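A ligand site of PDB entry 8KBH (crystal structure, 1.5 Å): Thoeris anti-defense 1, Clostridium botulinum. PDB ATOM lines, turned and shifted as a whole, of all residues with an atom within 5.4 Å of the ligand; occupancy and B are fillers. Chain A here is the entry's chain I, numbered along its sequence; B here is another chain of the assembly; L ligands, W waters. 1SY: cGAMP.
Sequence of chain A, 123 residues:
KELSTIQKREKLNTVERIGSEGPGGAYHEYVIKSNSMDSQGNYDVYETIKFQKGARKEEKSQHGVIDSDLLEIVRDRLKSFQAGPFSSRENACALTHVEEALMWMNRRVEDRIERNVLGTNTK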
ATOM      1  N   PRO A  23      10.561  24.988  18.310  1.00  0.00           N
ATOM      2  CA  PRO A  23      11.224  25.156  17.005  1.00  0.00           C
ATOM      3  C   PRO A  23      11.944  23.881  16.566  1.00  0.00           C
ATOM      4  O   PRO A  23      12.629  23.227  17.362  1.00  0.00           O
ATOM      5  CB  PRO A  23      12.225  26.295  17.256  1.00  0.00           C
ATOM      6  CG  PRO A  23      11.704  27.014  18.470  1.00  0.00           C
ATOM      7  CD  PRO A  23      11.036  25.971  19.306  1.00  0.00           C
ATOM      8  N   GLY A  24      11.765  23.530  15.292  1.00  0.00           N
ATOM      9  CA  GLY A  24      12.326  22.305  14.744  1.00  0.00           C
ATOM     10  C   GLY A  24      11.614  21.040  15.153  1.00  0.00           C
ATOM     11  O   GLY A  24      12.011  19.947  14.691  1.00  0.00           O
ATOM     12  N   GLY A  25      10.575  21.130  15.970  1.00  0.00           N
ATOM     13  CA  GLY A  25       9.820  19.981  16.412  1.00  0.00           C
ATOM     14  C   GLY A  25      10.327  19.318  17.670  1.00  0.00           C
ATOM     15  O   GLY A  25       9.862  18.215  18.000  1.00  0.00           O
ATOM     16  N   HIS A  28      12.609  21.643  24.551  1.00  0.00           N
ATOM     17  CA  HIS A  28      13.737  22.459  24.966  1.00  0.00           C
ATOM     18  C   HIS A  28      13.875  22.517  26.477  1.00  0.00           C
ATOM     19  O   HIS A  28      14.598  23.360  27.016  1.00  0.00           O
ATOM     20  CB  HIS A  28      13.606  23.867  24.386  1.00  0.00           C
ATOM     21  CG  HIS A  28      13.646  23.899  22.886  1.00  0.00           C
ATOM     22  ND1 HIS A  28      12.605  23.426  22.116  1.00  0.00           N
ATOM     23  CD2 HIS A  28      14.618  24.292  22.020  1.00  0.00           C
ATOM     24  CE1 HIS A  28      12.915  23.567  20.840  1.00  0.00           C
ATOM     25  NE2 HIS A  28      14.135  24.081  20.750  1.00  0.00           N
ATOM     26  N   GLN A  52      18.745  26.425  24.705  1.00  0.00           N
ATOM     27  CA  GLN A  52      18.523  27.560  23.818  1.00  0.00           C
ATOM     28  C   GLN A  52      17.320  27.305  22.913  1.00  0.00           C
ATOM     29  O   GLN A  52      17.289  26.322  22.176  1.00  0.00           O
ATOM     30  CB  GLN A  52      19.776  27.812  22.981  1.00  0.00           C
ATOM     31  CG  GLN A  52      19.718  29.114  22.187  1.00  0.00           C
ATOM     32  CD  GLN A  52      19.721  30.327  23.084  1.00  0.00           C
ATOM     33  OE1 GLN A  52      20.406  30.347  24.106  1.00  0.00           O
ATOM     34  NE2 GLN A  52      18.948  31.340  22.722  1.00  0.00           N
ATOM     35  N   LYS A  53      16.328  28.179  22.990  1.00  0.00           N
ATOM     36  CA  LYS A  53      15.095  28.060  22.213  1.00  0.00           C
ATOM     37  C   LYS A  53      14.831  29.421  21.592  1.00  0.00           C
ATOM     38  O   LYS A  53      14.444  30.360  22.287  1.00  0.00           O
ATOM     39  CB  LYS A  53      13.936  27.587  23.102  1.00  0.00           C
ATOM     40  CG  LYS A  53      12.584  27.344  22.414  1.00  0.00           C
ATOM     41  CD  LYS A  53      11.483  27.157  23.484  1.00  0.00           C
ATOM     42  CE  LYS A  53      10.107  26.906  22.880  1.00  0.00           C
ATOM     43  NZ  LYS A  53       9.221  26.103  23.794  1.00  0.00           N
ATOM     44  N   GLY A  54      15.044  29.523  20.279  1.00  0.00           N
ATOM     45  CA  GLY A  54      15.149  30.817  19.623  1.00  0.00           C
ATOM     46  C   GLY A  54      16.582  31.303  19.575  1.00  0.00           C
ATOM     47  O   GLY A  54      17.430  30.910  20.376  1.00  0.00           O
ATOM     48  N   ALA A  55      16.845  32.181  18.615  1.00  0.00           N
ATOM     49  CA  ALA A  55      18.204  32.667  18.388  1.00  0.00           C
ATOM     50  C   ALA A  55      18.743  33.441  19.588  1.00  0.00           C
ATOM     51  O   ALA A  55      18.004  34.169  20.263  1.00  0.00           O
ATOM     52  CB  ALA A  55      18.242  33.541  17.143  1.00  0.00           C
ATOM     53  N   ARG A  56      20.035  33.275  19.841  1.00  0.00           N
ATOM     54  CA  ARG A  56      20.684  33.921  20.980  1.00  0.00           C
ATOM     55  C   ARG A  56      20.750  35.437  20.816  1.00  0.00           C
ATOM     56  O   ARG A  56      20.792  36.168  21.820  1.00  0.00           O
ATOM     57  CB  ARG A  56      22.075  33.331  21.169  1.00  0.00           C
ATOM     58  CG  ARG A  56      22.985  34.026  22.187  1.00  0.00           C
ATOM     59  CD  ARG A  56      22.474  33.899  23.612  1.00  0.00           C
ATOM     60  NE  ARG A  56      22.405  32.526  24.099  1.00  0.00           N
ATOM     61  CZ  ARG A  56      23.438  31.844  24.567  1.00  0.00           C
ATOM     62  NH1 ARG A  56      24.652  32.388  24.602  1.00  0.00           N
ATOM     63  NH2 ARG A  56      23.271  30.599  24.992  1.00  0.00           N
ATOM     64  N   ILE A  66      23.219  24.054  24.980  1.00  0.00           N
ATOM     65  CA  ILE A  66      23.125  23.416  23.676  1.00  0.00           C
ATOM     66  C   ILE A  66      23.769  22.048  23.844  1.00  0.00           C
ATOM     67  O   ILE A  66      24.549  21.816  24.764  1.00  0.00           O
ATOM     68  CB  ILE A  66      23.805  24.264  22.574  1.00  0.00           C
ATOM     69  CG1 ILE A  66      23.224  23.945  21.190  1.00  0.00           C
ATOM     70  CG2 ILE A  66      25.317  24.094  22.618  1.00  0.00           C
ATOM     71  CD1 ILE A  66      21.731  24.164  21.100  1.00  0.00           C
ATOM     72  N   ASP A  67      23.413  21.124  22.949  1.00  0.00           N
ATOM     73  CA  ASP A  67      23.733  19.705  23.187  1.00  0.00           C
ATOM     74  C   ASP A  67      25.243  19.447  23.238  1.00  0.00           C
ATOM     75  O   ASP A  67      25.701  18.577  23.993  1.00  0.00           O
ATOM     76  CB  ASP A  67      23.080  18.844  22.117  1.00  0.00           C
ATOM     77  CG  ASP A  67      21.618  19.203  21.927  1.00  0.00           C
ATOM     78  OD1 ASP A  67      21.358  20.300  21.364  1.00  0.00           O
ATOM     79  OD2 ASP A  67      20.758  18.425  22.370  1.00  0.00           O
ATOM     80  N   ARG A 108      28.020  20.308  11.553  1.00  0.00           N
ATOM     81  CA  ARG A 108      26.750  20.982  11.330  1.00  0.00           C
ATOM     82  C   ARG A 108      26.917  22.503  11.485  1.00  0.00           C
ATOM     83  O   ARG A 108      26.509  23.261  10.653  1.00  0.00           O
ATOM     84  CB  ARG A 108      25.699  20.502  12.328  1.00  0.00           C
ATOM     85  CG  ARG A 108      24.328  21.092  12.076  1.00  0.00           C
ATOM     86  CD  ARG A 108      23.346  20.688  13.128  1.00  0.00           C
ATOM     87  NE  ARG A 108      22.122  21.447  12.996  1.00  0.00           N
ATOM     88  CZ  ARG A 108      21.865  22.579  13.647  1.00  0.00           C
ATOM     89  NH1 ARG A 108      22.736  23.091  14.494  1.00  0.00           N
ATOM     90  NH2 ARG A 108      20.742  23.212  13.448  1.00  0.00           N
ATOM     91  N   VAL A 109      27.526  22.921  12.581  1.00  0.00           N
ATOM     92  CA  VAL A 109      27.646  24.370  12.794  1.00  0.00           C
ATOM     93  C   VAL A 109      28.436  25.008  11.655  1.00  0.00           C
ATOM     94  O   VAL A 109      28.029  26.031  11.097  1.00  0.00           O
ATOM     95  CB  VAL A 109      28.297  24.663  14.158  1.00  0.00           C
ATOM     96  CG1 VAL A 109      28.709  26.134  14.266  1.00  0.00           C
ATOM     97  CG2 VAL A 109      27.352  24.289  15.276  1.00  0.00           C
ATOM     98  N   ARG A 112      26.470  25.145   8.448  1.00  0.00           N
ATOM     99  CA  ARG A 112      25.459  26.201   8.491  1.00  0.00           C
ATOM    100  C   ARG A 112      26.105  27.573   8.355  1.00  0.00           C
ATOM    101  O   ARG A 112      25.528  28.465   7.724  1.00  0.00           O
ATOM    102  CB  ARG A 112      24.643  26.053   9.774  1.00  0.00           C
ATOM    103  CG  ARG A 112      23.773  24.776   9.765  1.00  0.00           C
ATOM    104  CD  ARG A 112      22.938  24.670  11.019  1.00  0.00           C
ATOM    105  NE  ARG A 112      21.832  25.625  11.020  1.00  0.00           N
ATOM    106  CZ  ARG A 112      20.739  25.504  10.274  1.00  0.00           C
ATOM    107  NH1 ARG A 112      20.597  24.470   9.445  1.00  0.00           N
ATOM    108  NH2 ARG A 112      19.787  26.422  10.345  1.00  0.00           N
ATOM    109  N   VAL A 117      23.226  30.090   7.111  1.00  0.00           N
ATOM    110  CA  VAL A 117      21.961  29.742   7.734  1.00  0.00           C
ATOM    111  C   VAL A 117      22.071  29.518   9.236  1.00  0.00           C
ATOM    112  O   VAL A 117      21.033  29.278   9.877  1.00  0.00           O
ATOM    113  CB  VAL A 117      21.305  28.520   7.069  1.00  0.00           C
ATOM    114  CG1 VAL A 117      21.165  28.738   5.555  1.00  0.00           C
ATOM    115  CG2 VAL A 117      22.119  27.239   7.348  1.00  0.00           C
ATOM    116  N   LEU A 118      23.266  29.564   9.826  1.00  0.00           N
ATOM    117  CA  LEU A 118      23.403  29.429  11.286  1.00  0.00           C
ATOM    118  C   LEU A 118      22.580  30.491  12.007  1.00  0.00           C
ATOM    119  O   LEU A 118      22.663  31.682  11.682  1.00  0.00           O
ATOM    120  CB  LEU A 118      24.872  29.541  11.707  1.00  0.00           C
ATOM    121  CG  LEU A 118      25.180  29.319  13.194  1.00  0.00           C
ATOM    122  CD1 LEU A 118      24.897  27.869  13.603  1.00  0.00           C
ATOM    123  CD2 LEU A 118      26.602  29.698  13.548  1.00  0.00           C
ATOM    124  N   GLY A 119      21.797  30.063  12.998  1.00  0.00           N
ATOM    125  CA  GLY A 119      20.938  30.954  13.725  1.00  0.00           C
ATOM    126  C   GLY A 119      19.634  31.307  13.025  1.00  0.00           C
ATOM    127  O   GLY A 119      18.988  32.282  13.409  1.00  0.00           O
ATOM    128  N   THR A 120      19.262  30.544  12.000  1.00  0.00           N
ATOM    129  CA  THR A 120      18.029  30.763  11.257  1.00  0.00           C
ATOM    130  C   THR A 120      17.229  29.469  11.232  1.00  0.00           C
ATOM    131  O   THR A 120      17.804  28.377  11.279  1.00  0.00           O
ATOM    132  CB  THR A 120      18.284  31.234   9.824  1.00  0.00           C
ATOM    133  OG1 THR A 120      18.763  30.147   9.034  1.00  0.00           O
ATOM    134  CG2 THR A 120      19.324  32.366   9.787  1.00  0.00           C
ATOM    135  N   ASN A 121      15.912  29.609  11.148  1.00  0.00           N
ATOM    136  CA  ASN A 121      14.990  28.474  11.158  1.00  0.00           C
ATOM    137  C   ASN A 121      14.874  27.953   9.732  1.00  0.00           C
ATOM    138  O   ASN A 121      13.914  28.214   9.008  1.00  0.00           O
ATOM    139  CB  ASN A 121      13.645  28.901  11.715  1.00  0.00           C
ATOM    140  CG  ASN A 121      13.712  29.183  13.194  1.00  0.00           C
ATOM    141  OD1 ASN A 121      14.612  28.681  13.881  1.00  0.00           O
ATOM    142  ND2 ASN A 121      12.807  30.010  13.679  1.00  0.00           N
ATOM    143  N   THR A 122      15.913  27.239   9.311  1.00  0.00           N
ATOM    144  CA  THR A 122      15.900  26.714   7.951  1.00  0.00           C
ATOM    145  C   THR A 122      16.805  25.495   7.927  1.00  0.00           C
ATOM    146  O   THR A 122      17.727  25.397   8.728  1.00  0.00           O
ATOM    147  CB  THR A 122      16.381  27.780   6.963  1.00  0.00           C
ATOM    148  OG1 THR A 122      15.673  29.001   7.222  1.00  0.00           O
ATOM    149  CG2 THR A 122      16.076  27.327   5.528  1.00  0.00           C
ATOM    150  N   GLN B   9      34.376  22.164  19.097  1.00  0.00           N
ATOM    151  CA  GLN B   9      33.954  23.379  18.381  1.00  0.00           C
ATOM    152  C   GLN B   9      34.825  24.564  18.781  1.00  0.00           C
ATOM    153  O   GLN B   9      35.066  24.808  19.964  1.00  0.00           O
ATOM    154  CB  GLN B   9      32.487  23.680  18.693  1.00  0.00           C
ATOM    155  CG  GLN B   9      31.923  24.914  17.990  1.00  0.00           C
ATOM    156  CD  GLN B   9      30.475  25.167  18.381  1.00  0.00           C
ATOM    157  OE1 GLN B   9      29.892  24.389  19.122  1.00  0.00           O
ATOM    158  NE2 GLN B   9      29.894  26.257  17.880  1.00  0.00           N
ATOM    159  N   GLU B  12      31.961  30.303  16.786  1.00  0.00           N
ATOM    160  CA  GLU B  12      30.532  30.570  17.012  1.00  0.00           C
ATOM    161  C   GLU B  12      29.969  29.785  18.201  1.00  0.00           C
ATOM    162  O   GLU B  12      28.871  29.252  18.130  1.00  0.00           O
ATOM    163  CB  GLU B  12      29.704  30.292  15.764  1.00  0.00           C
ATOM    164  CG  GLU B  12      29.783  31.355  14.707  1.00  0.00           C
ATOM    165  CD  GLU B  12      29.303  32.712  15.205  1.00  0.00           C
ATOM    166  OE1 GLU B  12      28.325  32.750  15.987  1.00  0.00           O
ATOM    167  OE2 GLU B  12      29.890  33.729  14.812  1.00  0.00           O
ATOM    168  N   LYS B  13      30.717  29.734  19.303  1.00  0.00           N
ATOM    169  CA  LYS B  13      30.243  29.006  20.476  1.00  0.00           C
ATOM    170  C   LYS B  13      29.194  29.822  21.213  1.00  0.00           C
ATOM    171  O   LYS B  13      29.360  31.025  21.432  1.00  0.00           O
ATOM    172  CB  LYS B  13      31.413  28.671  21.406  1.00  0.00           C
ATOM    173  CG  LYS B  13      32.402  27.688  20.817  1.00  0.00           C
ATOM    174  CD  LYS B  13      33.600  27.497  21.725  1.00  0.00           C
ATOM    175  CE  LYS B  13      33.183  26.824  23.014  1.00  0.00           C
ATOM    176  NZ  LYS B  13      34.241  26.824  24.049  1.00  0.00           N
ATOM    177  N   LEU B  14      28.091  29.168  21.585  1.00  0.00           N
ATOM    178  CA  LEU B  14      27.092  29.830  22.428  1.00  0.00           C
ATOM    179  C   LEU B  14      27.559  29.952  23.866  1.00  0.00           C
ATOM    180  O   LEU B  14      27.327  30.979  24.515  1.00  0.00           O
ATOM    181  CB  LEU B  14      25.771  29.074  22.396  1.00  0.00           C
ATOM    182  CG  LEU B  14      24.922  29.109  21.130  1.00  0.00           C
ATOM    183  CD1 LEU B  14      23.788  28.091  21.237  1.00  0.00           C
ATOM    184  CD2 LEU B  14      24.392  30.530  20.925  1.00  0.00           C
ATOM    185  N   ARG B  79      16.388  14.788  21.596  1.00  0.00           N
ATOM    186  CA  ARG B  79      16.305  16.014  20.809  1.00  0.00           C
ATOM    187  C   ARG B  79      16.735  15.757  19.362  1.00  0.00           C
ATOM    188  O   ARG B  79      16.094  16.256  18.430  1.00  0.00           O
ATOM    189  CB  ARG B  79      17.118  17.128  21.443  1.00  0.00           C
ATOM    190  CG  ARG B  79      16.408  17.807  22.627  1.00  0.00           C
ATOM    191  CD  ARG B  79      17.325  18.710  23.443  1.00  0.00           C
ATOM    192  NE  ARG B  79      18.179  19.568  22.614  1.00  0.00           N
ATOM    193  CZ  ARG B  79      17.821  20.746  22.094  1.00  0.00           C
ATOM    194  NH1 ARG B  79      16.605  21.236  22.313  1.00  0.00           N
ATOM    195  NH2 ARG B  79      18.693  21.426  21.351  1.00  0.00           N
ATOM    196  N   LEU B  80      17.783  14.972  19.149  1.00  0.00           N
ATOM    197  CA  LEU B  80      18.215  14.732  17.775  1.00  0.00           C
ATOM    198  C   LEU B  80      17.159  13.938  17.017  1.00  0.00           C
ATOM    199  O   LEU B  80      16.885  14.240  15.847  1.00  0.00           O
ATOM    200  CB  LEU B  80      19.565  14.027  17.748  1.00  0.00           C
ATOM    201  CG  LEU B  80      20.776  14.886  18.098  1.00  0.00           C
ATOM    202  CD1 LEU B  80      21.950  13.958  18.384  1.00  0.00           C
ATOM    203  CD2 LEU B  80      21.164  15.880  16.985  1.00  0.00           C
ATOM    204  N   PHE B  83      14.532  16.523  16.060  1.00  0.00           N
ATOM    205  CA  PHE B  83      15.004  17.347  14.944  1.00  0.00           C
ATOM    206  C   PHE B  83      14.987  16.580  13.644  1.00  0.00           C
ATOM    207  O   PHE B  83      14.732  17.151  12.580  1.00  0.00           O
ATOM    208  CB  PHE B  83      16.417  17.850  15.214  1.00  0.00           C
ATOM    209  CG  PHE B  83      16.508  18.884  16.293  1.00  0.00           C
ATOM    210  CD1 PHE B  83      15.624  19.943  16.319  1.00  0.00           C
ATOM    211  CD2 PHE B  83      17.472  18.793  17.287  1.00  0.00           C
ATOM    212  CE1 PHE B  83      15.698  20.884  17.300  1.00  0.00           C
ATOM    213  CE2 PHE B  83      17.548  19.738  18.284  1.00  0.00           C
ATOM    214  CZ  PHE B  83      16.661  20.793  18.294  1.00  0.00           C
ATOM    215  N   PHE B  88      14.085  20.766   9.949  1.00  0.00           N
ATOM    216  CA  PHE B  88      15.475  21.185   9.883  1.00  0.00           C
ATOM    217  C   PHE B  88      16.408  19.993  10.114  1.00  0.00           C
ATOM    218  O   PHE B  88      17.452  20.114  10.769  1.00  0.00           O
ATOM    219  CB  PHE B  88      15.731  22.306  10.884  1.00  0.00           C
ATOM    220  CG  PHE B  88      14.729  23.418  10.795  1.00  0.00           C
ATOM    221  CD1 PHE B  88      14.256  23.840   9.561  1.00  0.00           C
ATOM    222  CD2 PHE B  88      14.204  23.991  11.943  1.00  0.00           C
ATOM    223  CE1 PHE B  88      13.316  24.840   9.485  1.00  0.00           C
ATOM    224  CE2 PHE B  88      13.256  25.012  11.868  1.00  0.00           C
ATOM    225  CZ  PHE B  88      12.819  25.423  10.632  1.00  0.00           C
ATOM    226  N   SER B  89      16.033  18.845   9.591  1.00  0.00           N
ATOM    227  CA  SER B  89      16.861  17.659   9.688  1.00  0.00           C
ATOM    228  C   SER B  89      18.123  17.810   8.839  1.00  0.00           C
ATOM    229  O   SER B  89      18.213  18.674   7.960  1.00  0.00           O
ATOM    230  CB  SER B  89      16.060  16.430   9.262  1.00  0.00           C
ATOM    231  OG  SER B  89      15.481  16.637   7.978  1.00  0.00           O
ATOM    232  N   ASN B  93      23.222  15.798  11.638  1.00  0.00           N
ATOM    233  CA  ASN B  93      22.418  15.332  12.770  1.00  0.00           C
ATOM    234  C   ASN B  93      22.362  13.804  12.845  1.00  0.00           C
ATOM    235  O   ASN B  93      22.421  13.235  13.939  1.00  0.00           O
ATOM    236  CB  ASN B  93      20.983  15.845  12.652  1.00  0.00           C
ATOM    237  CG  ASN B  93      20.800  17.255  13.139  1.00  0.00           C
ATOM    238  OD1 ASN B  93      21.719  17.930  13.605  1.00  0.00           O
ATOM    239  ND2 ASN B  93      19.562  17.707  13.038  1.00  0.00           N
HETATM  240  C2  1SY L   1      20.270  22.521  17.363  1.00  0.00           C
HETATM  241  N01 1SY L   1      21.462  19.519  15.965  1.00  0.00           N
HETATM  242  C6  1SY L   1      20.720  20.606  16.153  1.00  0.00           C
HETATM  243  N1  1SY L   1      21.026  21.434  17.173  1.00  0.00           N
HETATM  244  N3  1SY L   1      19.215  22.942  16.671  1.00  0.00           N
HETATM  245  C4  1SY L   1      18.942  22.095  15.670  1.00  0.00           C
HETATM  246  C5  1SY L   1      19.618  20.937  15.354  1.00  0.00           C
HETATM  247  N7  1SY L   1      19.051  20.320  14.250  1.00  0.00           N
HETATM  248  C8  1SY L   1      18.034  21.103  13.920  1.00  0.00           C
HETATM  249  N9  1SY L   1      17.909  22.205  14.746  1.00  0.00           N
HETATM  250  C1' 1SY L   1      16.865  23.223  14.592  1.00  0.00           C
HETATM  251  C2' 1SY L   1      16.396  23.921  15.866  1.00  0.00           C
HETATM  252  O2' 1SY L   1      14.979  24.055  15.833  1.00  0.00           O
HETATM  253  C3' 1SY L   1      17.138  25.249  15.792  1.00  0.00           C
HETATM  254  C4' 1SY L   1      17.190  25.524  14.291  1.00  0.00           C
HETATM  255  C16 1SY L   1      18.286  26.461  13.838  1.00  0.00           C
HETATM  256  O17 1SY L   1      19.549  25.917  14.296  1.00  0.00           O
HETATM  257  P18 1SY L   1      20.933  26.715  14.235  1.00  0.00           P
HETATM  258  O19 1SY L   1      21.915  25.734  14.773  1.00  0.00           O
HETATM  259  O20 1SY L   1      20.606  27.896  15.269  1.00  0.00           O
HETATM  260  C21 1SY L   1      20.192  27.595  16.581  1.00  0.00           C
HETATM  261  C22 1SY L   1      19.038  28.489  17.037  1.00  0.00           C
HETATM  262  O23 1SY L   1      19.390  29.802  16.623  1.00  0.00           O
HETATM  263  C24 1SY L   1      19.188  28.446  18.565  1.00  0.00           C
HETATM  264  C25 1SY L   1      18.199  27.552  19.289  1.00  0.00           C
HETATM  265  O26 1SY L   1      17.876  26.412  18.466  1.00  0.00           O
HETATM  266  P27 1SY L   1      16.338  26.229  18.099  1.00  0.00           P
HETATM  267  O28 1SY L   1      16.464  26.272  16.499  1.00  0.00           O
HETATM  268  O29 1SY L   1      15.809  24.931  18.628  1.00  0.00           O
HETATM  269  O30 1SY L   1      15.599  27.472  18.446  1.00  0.00           O
HETATM  270  O31 1SY L   1      20.534  27.989  18.829  1.00  0.00           O
HETATM  271  C32 1SY L   1      21.224  28.059  17.592  1.00  0.00           C
HETATM  272  N33 1SY L   1      22.444  27.272  17.685  1.00  0.00           N
HETATM  273  C34 1SY L   1      22.590  25.912  17.818  1.00  0.00           C
HETATM  274  N35 1SY L   1      23.844  25.529  17.903  1.00  0.00           N
HETATM  275  C36 1SY L   1      23.715  27.792  17.665  1.00  0.00           C
HETATM  276  C37 1SY L   1      24.582  26.704  17.813  1.00  0.00           C
HETATM  277  C38 1SY L   1      26.002  27.011  17.825  1.00  0.00           C
HETATM  278  N39 1SY L   1      26.439  28.295  17.706  1.00  0.00           N
HETATM  279  C40 1SY L   1      25.571  29.291  17.579  1.00  0.00           C
HETATM  280  N41 1SY L   1      25.990  30.549  17.476  1.00  0.00           N
HETATM  281  N42 1SY L   1      24.226  29.070  17.562  1.00  0.00           N
HETATM  282  O43 1SY L   1      26.857  26.144  17.946  1.00  0.00           O
HETATM  283  O44 1SY L   1      21.159  27.268  12.872  1.00  0.00           O
HETATM  284  O4' 1SY L   1      17.378  24.220  13.711  1.00  0.00           O
HETATM  285  O   HOH W   1      23.681  32.686  18.017  1.00  0.00           O
HETATM  286  O   HOH W   2      27.768  26.400  20.755  1.00  0.00           O
HETATM  287  O   HOH W   3      17.044  29.969  14.905  1.00  0.00           O
HETATM  288  O   HOH W   4      24.192  19.488  16.939  1.00  0.00           O
HETATM  289  O   HOH W   5      22.822  20.873  19.103  1.00  0.00           O
HETATM  290  O   HOH W   6      14.624  28.948  16.445  1.00  0.00           O
HETATM  291  O   HOH W   7      17.726  23.921  20.595  1.00  0.00           O
HETATM  292  O   HOH W   8      21.520  31.418  17.874  1.00  0.00           O
HETATM  293  O   HOH W   9      18.802  23.106  11.800  1.00  0.00           O
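NE of Arg 112 is in salt-bridge range of O44 of the ligand.
O of Glu 12 of chain B lies within hydrogen-bond range of N41 of the ligand (3.2 Å).
An oxygen (O19) of the ligand lies within salt-bridge range of the guanidinium group (NH1) of Arg 108.
The backbone NH (N) of Gly 54 lies within hydrogen-bond range of an oxygen (O30) of the ligand, at 2.8 Å.
A ring nitrogen (NE2) of His 28 sits at hydrogen-bond distance from an oxygen (O29) of the ligand.
A nitrogen (N01) of the ligand lies within hydrogen-bond range of the side-chain amide oxygen (OD1) of Asn 93 of chain B, at 2.9 Å.
The backbone NH (N) of Gly 119 sits at hydrogen-bond distance from an oxygen (O44) of the ligand (2.9 Å).
The backbone carbonyl oxygen (O) of Pro 23 sits at hydrogen-bond distance from an oxygen (O2') of the ligand, 2.9 Å away.
The side-chain amide nitrogen (NE2) of Gln 9 of chain B sits at hydrogen-bond distance from an oxygen (O43) of the ligand, at 3.0 Å.
An oxygen (O2') of the ligand lies within hydrogen-bond range of the backbone NH of Gly 24 (3.3 Å).
O of Thr 120 lies within hydrogen-bond range of NH2 of Arg 112, 2.9 Å away.
The backbone carbonyl oxygen of Arg 112 is in hydrogen-bond range of the backbone NH of Leu 118.
The backbone carbonyl oxygen of Arg 112 sits at hydrogen-bond distance from the backbone NH of Val 117 (2.9 Å).
The backbone carbonyl oxygen (O) of Thr 122 lies within hydrogen-bond range of the guanidinium group (NH2) of Arg 112 (2.8 Å).
The backbone carbonyl oxygen of Gly 54 lies within hydrogen-bond range of the side-chain amide nitrogen of Gln 52, at 2.8 Å.
The side-chain hydroxyl of Thr 120 lies within hydrogen-bond range of the backbone carbonyl oxygen of Val 117 (2.6 Å).
OE1 of Gln 52 is in hydrogen-bond range of NE of Arg 56 (3.0 Å).
The backbone carbonyl oxygen (O) of Leu 14 of chain B lies within hydrogen-bond range of the guanidinium group (NH1) of Arg 56, at 3.0 Å.
Gln 52 touches the ligand.
Lys 53 touches the ligand (C to O30, 3.8 Å).
Ala 55 touches the ligand (CA to O23, 3.6 Å).
Ile 66 touches the ligand (CG1 to N35, 3.7 Å).
Val 109 touches the ligand (CG2 to O43, 3.3 Å).
Val 117 touches the ligand.
CA of Leu 118 touches O44 of the ligand (3.5 Å).
Thr 120 touches the ligand (O to C16, 3.2 Å).
Leu 14 of chain B touches the ligand.
Leu 80 of chain B touches the ligand.
Phe 83 of chain B touches the ligand.
O of Phe 88 of chain B touches C8 of the ligand (3.4 Å).
Water W9 lies within hydrogen-bond range of NH2 of Arg 108 (2.5 Å), O4' of the ligand (2.6 Å), NH1 of Arg 112 (3.3 Å) and O of Phe 88 of chain B (3.4 Å).
Water W6 lies within hydrogen-bond range of the side-chain amide oxygen (OD1) of Asn 121 (2.6 Å) and an oxygen (O30) of the ligand (2.7 Å).
Water W5 bridges a nitrogen (N1) of the ligand (2.7 Å) and the side-chain carboxylate (OD1) of Asp 67 (2.8 Å).
Water W3 lies within hydrogen-bond range of an oxygen (O23) of the ligand (2.9 Å), the side-chain amide oxygen of Asn 121 (2.9 Å) and the backbone carbonyl oxygen of Gly 119 (3.4 Å).
Water W7 lies within hydrogen-bond range of NH2 of Arg 79 of chain B (2.8 Å), O of Gln 52 (2.9 Å) and O29 of the ligand (2.9 Å).
Water W8 bridges O23 of the ligand (3.0 Å) and N of Arg 56 (3.1 Å).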
